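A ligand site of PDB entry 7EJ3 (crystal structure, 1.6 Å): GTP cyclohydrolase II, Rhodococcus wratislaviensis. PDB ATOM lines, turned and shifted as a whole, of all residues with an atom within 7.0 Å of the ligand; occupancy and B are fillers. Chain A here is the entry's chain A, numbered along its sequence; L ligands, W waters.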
ATOM      1  N   ARG A 247     -11.885  22.150   8.570  1.00  0.00           N
ATOM      2  CA  ARG A 247     -12.679  22.814   7.531  1.00  0.00           C
ATOM      3  C   ARG A 247     -12.504  24.312   7.690  1.00  0.00           C
ATOM      4  O   ARG A 247     -12.569  24.833   8.813  1.00  0.00           O
ATOM      5  CB  ARG A 247     -14.179  22.467   7.623  1.00  0.00           C
ATOM      6  CG  ARG A 247     -15.033  23.401   6.786  1.00  0.00           C
ATOM      7  CD  ARG A 247     -16.489  22.931   6.680  1.00  0.00           C
ATOM      8  NE  ARG A 247     -17.285  23.808   5.814  1.00  0.00           N
ATOM      9  CZ  ARG A 247     -17.199  23.827   4.489  1.00  0.00           C
ATOM     10  NH1 ARG A 247     -16.429  22.968   3.835  1.00  0.00           N
ATOM     11  NH2 ARG A 247     -17.886  24.737   3.804  1.00  0.00           N
ATOM     12  N   VAL A 248     -12.282  25.002   6.577  1.00  0.00           N
ATOM     13  CA  VAL A 248     -12.397  26.447   6.527  1.00  0.00           C
ATOM     14  C   VAL A 248     -13.744  26.772   5.893  1.00  0.00           C
ATOM     15  O   VAL A 248     -13.995  26.423   4.729  1.00  0.00           O
ATOM     16  CB  VAL A 248     -11.242  27.087   5.733  1.00  0.00           C
ATOM     17  CG1 VAL A 248     -11.457  28.615   5.672  1.00  0.00           C
ATOM     18  CG2 VAL A 248      -9.918  26.765   6.407  1.00  0.00           C
ATOM     19  N   HIS A 249     -14.592  27.421   6.677  1.00  0.00           N
ATOM     20  CA  HIS A 249     -15.971  27.720   6.315  1.00  0.00           C
ATOM     21  C   HIS A 249     -16.118  29.214   6.119  1.00  0.00           C
ATOM     22  O   HIS A 249     -15.767  29.995   7.020  1.00  0.00           O
ATOM     23  CB  HIS A 249     -16.902  27.239   7.423  1.00  0.00           C
ATOM     24  CG  HIS A 249     -18.342  27.257   7.056  1.00  0.00           C
ATOM     25  ND1 HIS A 249     -18.949  26.204   6.394  1.00  0.00           N
ATOM     26  CD2 HIS A 249     -19.310  28.183   7.251  1.00  0.00           C
ATOM     27  CE1 HIS A 249     -20.221  26.483   6.202  1.00  0.00           C
ATOM     28  NE2 HIS A 249     -20.470  27.684   6.717  1.00  0.00           N
ATOM     29  N   ASP A 250     -16.648  29.637   4.968  1.00  0.00           N
ATOM     30  CA  ASP A 250     -16.903  31.048   4.741  1.00  0.00           C
ATOM     31  C   ASP A 250     -18.346  31.399   5.102  1.00  0.00           C
ATOM     32  O   ASP A 250     -19.284  30.665   4.743  1.00  0.00           O
ATOM     33  CB  ASP A 250     -16.586  31.422   3.298  1.00  0.00           C
ATOM     34  CG  ASP A 250     -15.082  31.358   3.000  1.00  0.00           C
ATOM     35  OD1 ASP A 250     -14.292  31.861   3.836  1.00  0.00           O
ATOM     36  OD2 ASP A 250     -14.678  30.795   1.970  1.00  0.00           O
ATOM     37  N   THR A 264     -25.674  24.613   0.718  1.00  0.00           N
ATOM     38  CA  THR A 264     -25.106  23.500   1.481  1.00  0.00           C
ATOM     39  C   THR A 264     -24.400  23.931   2.753  1.00  0.00           C
ATOM     40  O   THR A 264     -23.816  23.080   3.426  1.00  0.00           O
ATOM     41  CB  THR A 264     -24.115  22.729   0.609  1.00  0.00           C
ATOM     42  OG1 THR A 264     -23.128  23.638   0.108  1.00  0.00           O
ATOM     43  CG2 THR A 264     -24.789  22.038  -0.570  1.00  0.00           C
ATOM     44  N   CYS A 265     -24.457  25.221   3.119  1.00  0.00           N
ATOM     45  CA  CYS A 265     -23.451  25.773   4.038  1.00  0.00           C
ATOM     46  C   CYS A 265     -23.551  25.189   5.440  1.00  0.00           C
ATOM     47  O   CYS A 265     -22.606  24.555   5.928  1.00  0.00           O
ATOM     48  CB  CYS A 265     -23.565  27.293   4.053  1.00  0.00           C
ATOM     49  SG  CYS A 265     -23.170  27.964   2.397  1.00  0.00           S
ATOM     50  N   TYR A 268     -22.678  21.521   5.697  1.00  0.00           N
ATOM     51  CA  TYR A 268     -21.260  21.188   5.610  1.00  0.00           C
ATOM     52  C   TYR A 268     -20.533  21.598   6.883  1.00  0.00           C
ATOM     53  O   TYR A 268     -19.658  20.874   7.370  1.00  0.00           O
ATOM     54  CB  TYR A 268     -20.631  21.851   4.383  1.00  0.00           C
ATOM     55  CG  TYR A 268     -19.594  21.007   3.647  1.00  0.00           C
ATOM     56  CD1 TYR A 268     -19.013  19.879   4.235  1.00  0.00           C
ATOM     57  CD2 TYR A 268     -19.208  21.340   2.351  1.00  0.00           C
ATOM     58  CE1 TYR A 268     -18.063  19.100   3.535  1.00  0.00           C
ATOM     59  CE2 TYR A 268     -18.273  20.599   1.658  1.00  0.00           C
ATOM     60  CZ  TYR A 268     -17.704  19.477   2.243  1.00  0.00           C
ATOM     61  OH  TYR A 268     -16.780  18.752   1.527  1.00  0.00           O
ATOM     62  N   ARG A 296     -19.664  35.074  -0.940  1.00  0.00           N
ATOM     63  CA  ARG A 296     -18.437  35.067  -1.730  1.00  0.00           C
ATOM     64  C   ARG A 296     -17.721  36.419  -1.649  1.00  0.00           C
ATOM     65  O   ARG A 296     -17.079  36.860  -2.604  1.00  0.00           O
ATOM     66  CB  ARG A 296     -18.734  34.692  -3.191  1.00  0.00           C
ATOM     67  CG  ARG A 296     -19.615  33.469  -3.325  1.00  0.00           C
ATOM     68  CD  ARG A 296     -19.761  33.104  -4.787  1.00  0.00           C
ATOM     69  NE  ARG A 296     -20.489  31.857  -4.973  1.00  0.00           N
ATOM     70  CZ  ARG A 296     -19.910  30.719  -5.333  1.00  0.00           C
ATOM     71  NH1 ARG A 296     -18.590  30.635  -5.462  1.00  0.00           N
ATOM     72  NH2 ARG A 296     -20.657  29.636  -5.527  1.00  0.00           N
ATOM     73  N   ASP A 334     -16.517  35.222  -7.776  1.00  0.00           N
ATOM     74  CA  ASP A 334     -16.149  35.011  -6.387  1.00  0.00           C
ATOM     75  C   ASP A 334     -15.057  36.008  -6.040  1.00  0.00           C
ATOM     76  O   ASP A 334     -14.120  36.178  -6.828  1.00  0.00           O
ATOM     77  CB  ASP A 334     -15.652  33.549  -6.235  1.00  0.00           C
ATOM     78  CG  ASP A 334     -15.494  33.104  -4.799  1.00  0.00           C
ATOM     79  OD1 ASP A 334     -14.751  33.729  -4.027  1.00  0.00           O
ATOM     80  OD2 ASP A 334     -16.080  32.079  -4.444  1.00  0.00           O
ATOM     81  N   ARG A 336     -13.566  35.944  -2.758  1.00  0.00           N
ATOM     82  CA  ARG A 336     -13.068  35.581  -1.433  1.00  0.00           C
ATOM     83  C   ARG A 336     -11.545  35.544  -1.341  1.00  0.00           C
ATOM     84  O   ARG A 336     -11.009  35.610  -0.224  1.00  0.00           O
ATOM     85  CB  ARG A 336     -13.649  34.228  -1.017  1.00  0.00           C
ATOM     86  CG  ARG A 336     -15.134  34.330  -0.716  1.00  0.00           C
ATOM     87  CD  ARG A 336     -15.651  32.986  -0.274  1.00  0.00           C
ATOM     88  NE  ARG A 336     -16.035  32.163  -1.424  1.00  0.00           N
ATOM     89  CZ  ARG A 336     -16.331  30.879  -1.337  1.00  0.00           C
ATOM     90  NH1 ARG A 336     -16.165  30.192  -0.215  1.00  0.00           N
ATOM     91  NH2 ARG A 336     -16.840  30.256  -2.406  1.00  0.00           N
ATOM     92  N   GLN A 338      -9.053  33.111  -1.685  1.00  0.00           N
ATOM     93  CA  GLN A 338      -8.537  32.070  -0.807  1.00  0.00           C
ATOM     94  C   GLN A 338      -7.013  32.087  -0.705  1.00  0.00           C
ATOM     95  O   GLN A 338      -6.470  31.378   0.150  1.00  0.00           O
ATOM     96  CB  GLN A 338      -9.017  30.705  -1.301  1.00  0.00           C
ATOM     97  CG  GLN A 338     -10.551  30.554  -1.412  1.00  0.00           C
ATOM     98  CD  GLN A 338     -11.286  30.662  -0.073  1.00  0.00           C
ATOM     99  OE1 GLN A 338     -10.676  30.615   0.995  1.00  0.00           O
ATOM    100  NE2 GLN A 338     -12.607  30.805  -0.139  1.00  0.00           N
ATOM    101  N   VAL A 357     -12.437  18.656   5.313  1.00  0.00           N
ATOM    102  CA  VAL A 357     -13.896  18.473   5.157  1.00  0.00           C
ATOM    103  C   VAL A 357     -14.375  19.675   4.307  1.00  0.00           C
ATOM    104  O   VAL A 357     -14.889  20.669   4.811  1.00  0.00           O
ATOM    105  CB  VAL A 357     -14.599  18.364   6.500  1.00  0.00           C
ATOM    106  CG1 VAL A 357     -16.097  18.051   6.326  1.00  0.00           C
ATOM    107  CG2 VAL A 357     -13.880  17.300   7.353  1.00  0.00           C
ATOM    108  N   SER A 358     -14.198  19.532   2.996  1.00  0.00           N
ATOM    109  CA  SER A 358     -14.332  20.620   2.043  1.00  0.00           C
ATOM    110  C   SER A 358     -14.166  20.011   0.652  1.00  0.00           C
ATOM    111  O   SER A 358     -13.533  18.959   0.508  1.00  0.00           O
ATOM    112  CB  SER A 358     -13.271  21.701   2.318  1.00  0.00           C
ATOM    113  OG  SER A 358     -13.279  22.762   1.389  1.00  0.00           O
ATOM    114  N   MET A 359     -14.728  20.664  -0.364  1.00  0.00           N
ATOM    115  CA  MET A 359     -14.582  20.238  -1.749  1.00  0.00           C
ATOM    116  C   MET A 359     -13.948  21.285  -2.650  1.00  0.00           C
ATOM    117  O   MET A 359     -13.313  20.920  -3.644  1.00  0.00           O
ATOM    118  CB  MET A 359     -15.951  19.856  -2.349  1.00  0.00           C
ATOM    119  CG  MET A 359     -16.564  18.658  -1.641  1.00  0.00           C
ATOM    120  SD  MET A 359     -18.359  18.630  -1.788  1.00  0.00           S
ATOM    121  CE  MET A 359     -18.584  18.362  -3.550  1.00  0.00           C
ATOM    122  N   SER A 360     -14.093  22.566  -2.313  1.00  0.00           N
ATOM    123  CA  SER A 360     -13.628  23.648  -3.172  1.00  0.00           C
ATOM    124  C   SER A 360     -12.218  23.414  -3.697  1.00  0.00           C
ATOM    125  O   SER A 360     -11.272  23.233  -2.924  1.00  0.00           O
ATOM    126  CB  SER A 360     -13.663  24.951  -2.389  1.00  0.00           C
ATOM    127  OG  SER A 360     -12.956  25.955  -3.093  1.00  0.00           O
ATOM    128  N   ASN A 361     -12.057  23.513  -5.030  1.00  0.00           N
ATOM    129  CA  ASN A 361     -10.707  23.455  -5.575  1.00  0.00           C
ATOM    130  C   ASN A 361      -9.923  24.710  -5.254  1.00  0.00           C
ATOM    131  O   ASN A 361      -8.685  24.654  -5.128  1.00  0.00           O
ATOM    132  CB  ASN A 361     -10.751  23.204  -7.087  1.00  0.00           C
ATOM    133  CG  ASN A 361     -11.499  24.301  -7.838  1.00  0.00           C
ATOM    134  OD1 ASN A 361     -12.640  24.630  -7.511  1.00  0.00           O
ATOM    135  ND2 ASN A 361     -10.853  24.866  -8.853  1.00  0.00           N
ATOM    136  N   MET A 362     -10.585  25.865  -5.103  1.00  0.00           N
ATOM    137  CA  MET A 362      -9.841  27.075  -4.780  1.00  0.00           C
ATOM    138  C   MET A 362      -9.250  26.990  -3.375  1.00  0.00           C
ATOM    139  O   MET A 362      -8.108  27.415  -3.158  1.00  0.00           O
ATOM    140  CB  MET A 362     -10.709  28.344  -4.909  1.00  0.00           C
ATOM    141  CG  MET A 362     -11.137  28.691  -6.332  1.00  0.00           C
ATOM    142  SD  MET A 362     -12.662  29.671  -6.389  1.00  0.00           S
ATOM    143  CE  MET A 362     -13.926  28.401  -6.132  1.00  0.00           C
ATOM    144  N   LYS A 363     -10.018  26.485  -2.403  1.00  0.00           N
ATOM    145  CA  LYS A 363      -9.464  26.330  -1.066  1.00  0.00           C
ATOM    146  C   LYS A 363      -8.360  25.284  -1.058  1.00  0.00           C
ATOM    147  O   LYS A 363      -7.304  25.489  -0.440  1.00  0.00           O
ATOM    148  CB  LYS A 363     -10.551  25.941  -0.068  1.00  0.00           C
ATOM    149  CG  LYS A 363     -11.602  27.022   0.171  1.00  0.00           C
ATOM    150  CD  LYS A 363     -12.612  26.581   1.213  1.00  0.00           C
ATOM    151  CE  LYS A 363     -13.869  27.454   1.200  1.00  0.00           C
ATOM    152  NZ  LYS A 363     -14.954  26.839   2.029  1.00  0.00           N
ATOM    153  N   GLU A 392     -26.664  24.536  -6.820  1.00  0.00           N
ATOM    154  CA  GLU A 392     -25.366  24.985  -6.298  1.00  0.00           C
ATOM    155  C   GLU A 392     -24.316  23.885  -6.352  1.00  0.00           C
ATOM    156  O   GLU A 392     -23.217  24.075  -6.904  1.00  0.00           O
ATOM    157  CB  GLU A 392     -25.543  25.482  -4.861  1.00  0.00           C
ATOM    158  CG  GLU A 392     -24.210  25.708  -4.129  1.00  0.00           C
ATOM    159  CD  GLU A 392     -24.208  25.119  -2.729  1.00  0.00           C
ATOM    160  OE1 GLU A 392     -23.126  24.780  -2.210  1.00  0.00           O
ATOM    161  OE2 GLU A 392     -25.298  25.016  -2.121  1.00  0.00           O
ATOM    162  N   ILE A 393     -24.602  22.726  -5.752  1.00  0.00           N
ATOM    163  CA  ILE A 393     -23.558  21.712  -5.613  1.00  0.00           C
ATOM    164  C   ILE A 393     -23.222  21.087  -6.967  1.00  0.00           C
ATOM    165  O   ILE A 393     -22.065  20.741  -7.223  1.00  0.00           O
ATOM    166  CB  ILE A 393     -23.950  20.668  -4.555  1.00  0.00           C
ATOM    167  CG1 ILE A 393     -22.701  19.963  -4.029  1.00  0.00           C
ATOM    168  CG2 ILE A 393     -24.931  19.655  -5.110  1.00  0.00           C
ATOM    169  CD1 ILE A 393     -21.737  20.887  -3.304  1.00  0.00           C
ATOM    170  N   LYS A 396     -20.955  23.544  -8.746  1.00  0.00           N
ATOM    171  CA  LYS A 396     -19.628  23.549  -8.137  1.00  0.00           C
ATOM    172  C   LYS A 396     -18.824  22.322  -8.551  1.00  0.00           C
ATOM    173  O   LYS A 396     -17.637  22.420  -8.869  1.00  0.00           O
ATOM    174  CB  LYS A 396     -19.740  23.609  -6.614  1.00  0.00           C
ATOM    175  CG  LYS A 396     -20.149  24.976  -6.089  1.00  0.00           C
ATOM    176  CD  LYS A 396     -20.356  24.973  -4.575  1.00  0.00           C
ATOM    177  CE  LYS A 396     -20.624  26.380  -4.078  1.00  0.00           C
ATOM    178  NZ  LYS A 396     -20.943  26.404  -2.622  1.00  0.00           N
ATOM    179  N   TYR A 401     -14.952  21.341  -8.167  1.00  0.00           N
ATOM    180  CA  TYR A 401     -14.946  20.949  -6.763  1.00  0.00           C
ATOM    181  C   TYR A 401     -14.787  19.438  -6.663  1.00  0.00           C
ATOM    182  O   TYR A 401     -15.347  18.685  -7.469  1.00  0.00           O
ATOM    183  CB  TYR A 401     -16.226  21.386  -6.057  1.00  0.00           C
ATOM    184  CG  TYR A 401     -16.284  22.837  -5.607  1.00  0.00           C
ATOM    185  CD1 TYR A 401     -15.839  23.863  -6.429  1.00  0.00           C
ATOM    186  CD2 TYR A 401     -16.845  23.177  -4.378  1.00  0.00           C
ATOM    187  CE1 TYR A 401     -15.917  25.191  -6.027  1.00  0.00           C
ATOM    188  CE2 TYR A 401     -16.927  24.487  -3.961  1.00  0.00           C
ATOM    189  CZ  TYR A 401     -16.465  25.497  -4.789  1.00  0.00           C
ATOM    190  OH  TYR A 401     -16.551  26.813  -4.378  1.00  0.00           O
ATOM    191  N   PHE A 402     -14.058  18.987  -5.642  1.00  0.00           N
ATOM    192  CA  PHE A 402     -13.781  17.574  -5.480  1.00  0.00           C
ATOM    193  C   PHE A 402     -15.064  16.761  -5.292  1.00  0.00           C
ATOM    194  O   PHE A 402     -15.940  17.130  -4.516  1.00  0.00           O
ATOM    195  CB  PHE A 402     -12.865  17.341  -4.283  1.00  0.00           C
ATOM    196  CG  PHE A 402     -12.699  15.889  -3.923  1.00  0.00           C
ATOM    197  CD1 PHE A 402     -11.794  15.089  -4.616  1.00  0.00           C
ATOM    198  CD2 PHE A 402     -13.466  15.301  -2.930  1.00  0.00           C
ATOM    199  CE1 PHE A 402     -11.646  13.754  -4.311  1.00  0.00           C
ATOM    200  CE2 PHE A 402     -13.323  13.962  -2.612  1.00  0.00           C
ATOM    201  CZ  PHE A 402     -12.414  13.184  -3.304  1.00  0.00           C
HETATM  202  P1  LIG L   1     -17.282  26.755  -0.761  1.00  0.00           P
HETATM  203  O1  LIG L   1     -17.115  27.615   0.469  1.00  0.00           O
HETATM  204  O2  LIG L   1     -16.778  27.471  -1.995  1.00  0.00           O
HETATM  205  O3  LIG L   1     -18.696  26.273  -0.974  1.00  0.00           O
HETATM  206  O4  LIG L   1     -16.290  25.463  -0.592  1.00  0.00           O
HETATM  207  P2  LIG L   1     -16.526  24.121   0.317  1.00  0.00           P
HETATM  208  O5  LIG L   1     -15.450  24.125   1.376  1.00  0.00           O
HETATM  209  O6  LIG L   1     -16.383  22.923  -0.603  1.00  0.00           O
HETATM  210  O7  LIG L   1     -17.872  24.171   0.972  1.00  0.00           O
HETATM  211  O   HOH W   1     -18.610  21.950  -1.777  1.00  0.00           O
HETATM  212  O   HOH W   2     -14.083  28.185  -2.329  1.00  0.00           O
HETATM  213  O   HOH W   3     -20.418  23.680  -0.878  1.00  0.00           O
HETATM  214  O   HOH W   4     -21.072  25.469   1.222  1.00  0.00           O
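The side-chain hydroxyl of Tyr 401 is in hydrogen-bond range of an oxygen (O2) of the ligand, 2.5 Å away. OG of Ser 358 is in hydrogen-bond range of O5 of the ligand, 2.6 Å away. O1 of the ligand lies within salt-bridge range of NZ of Lys 363, 2.8 Å away. NZ of Lys 396 is in salt-bridge range of O3 of the ligand (2.8 Å). The backbone NH (N) of Met 359 is in hydrogen-bond range of an oxygen (O6) of the ligand, 2.8 Å away. NH2 of Arg 336 lies within salt-bridge range of O2 of the ligand (2.8 Å). N of Ser 360 is in hydrogen-bond range of O6 of the ligand (2.9 Å). An oxygen (O7) of the ligand is in salt-bridge range of the guanidinium group (NH2) of Arg 247 (2.9 Å).
The backbone NH (N) of Tyr 401 sits at hydrogen-bond distance from the backbone carbonyl oxygen (O) of Lys 396 (3.0 Å). The side-chain amino group (NZ) of Lys 363 is in salt-bridge range of the side-chain carboxylate (OD2) of Asp 250. N of Met 359 lies close to OH of Tyr 268 (3.4 Å). O of Met 359 lies within hydrogen-bond range of N of Phe 402, 2.9 Å away. OD2 of Asp 250 is in salt-bridge range of NH1 of Arg 336. The guanidinium group of Arg 336 lies within salt-bridge range of the side-chain carboxylate of Asp 334, 2.8 Å away. The backbone NH (N) of Met 362 lies within hydrogen-bond range of the side-chain hydroxyl (OG) of Ser 360 (3.1 Å). NH1 of Arg 247 is in hydrogen-bond range of O of Val 357 (2.9 Å).
Tyr 268 touches the ligand (CD2 to O7, 3.4 Å). Hydrophobic or aromatic side chains within 4 Å of the ligand: Tyr 268, Met 359 and Tyr 401. Nine residues have an atom within 4 Å of the ligand: Arg 247, Tyr 268, Arg 336, Ser 358, Met 359, Ser 360, Lys 363, Lys 396 and Tyr 401.
Water W1 lies within hydrogen-bond range of an oxygen (O6) of the ligand (2.7 Å) and the side-chain sulfur (SD) of Met 359 (3.3 Å). Water W2 lies within hydrogen-bond range of the side-chain hydroxyl of Ser 360 (2.6 Å), an oxygen (O2) of the ligand (2.8 Å), the guanidinium group of Arg 336 (3.4 Å) and the side-chain hydroxyl of Tyr 401 (3.5 Å). Water W3 lies within hydrogen-bond range of the side-chain hydroxyl (OG1) of Thr 264, an oxygen (O3) of the ligand, the side-chain carboxylate (OE1) of Glu 392 and the side-chain amino group (NZ) of Lys 396. Water W4 lies within hydrogen-bond range of OG1 of Thr 264 (3.0 Å) and O3 of the ligand (3.3 Å).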
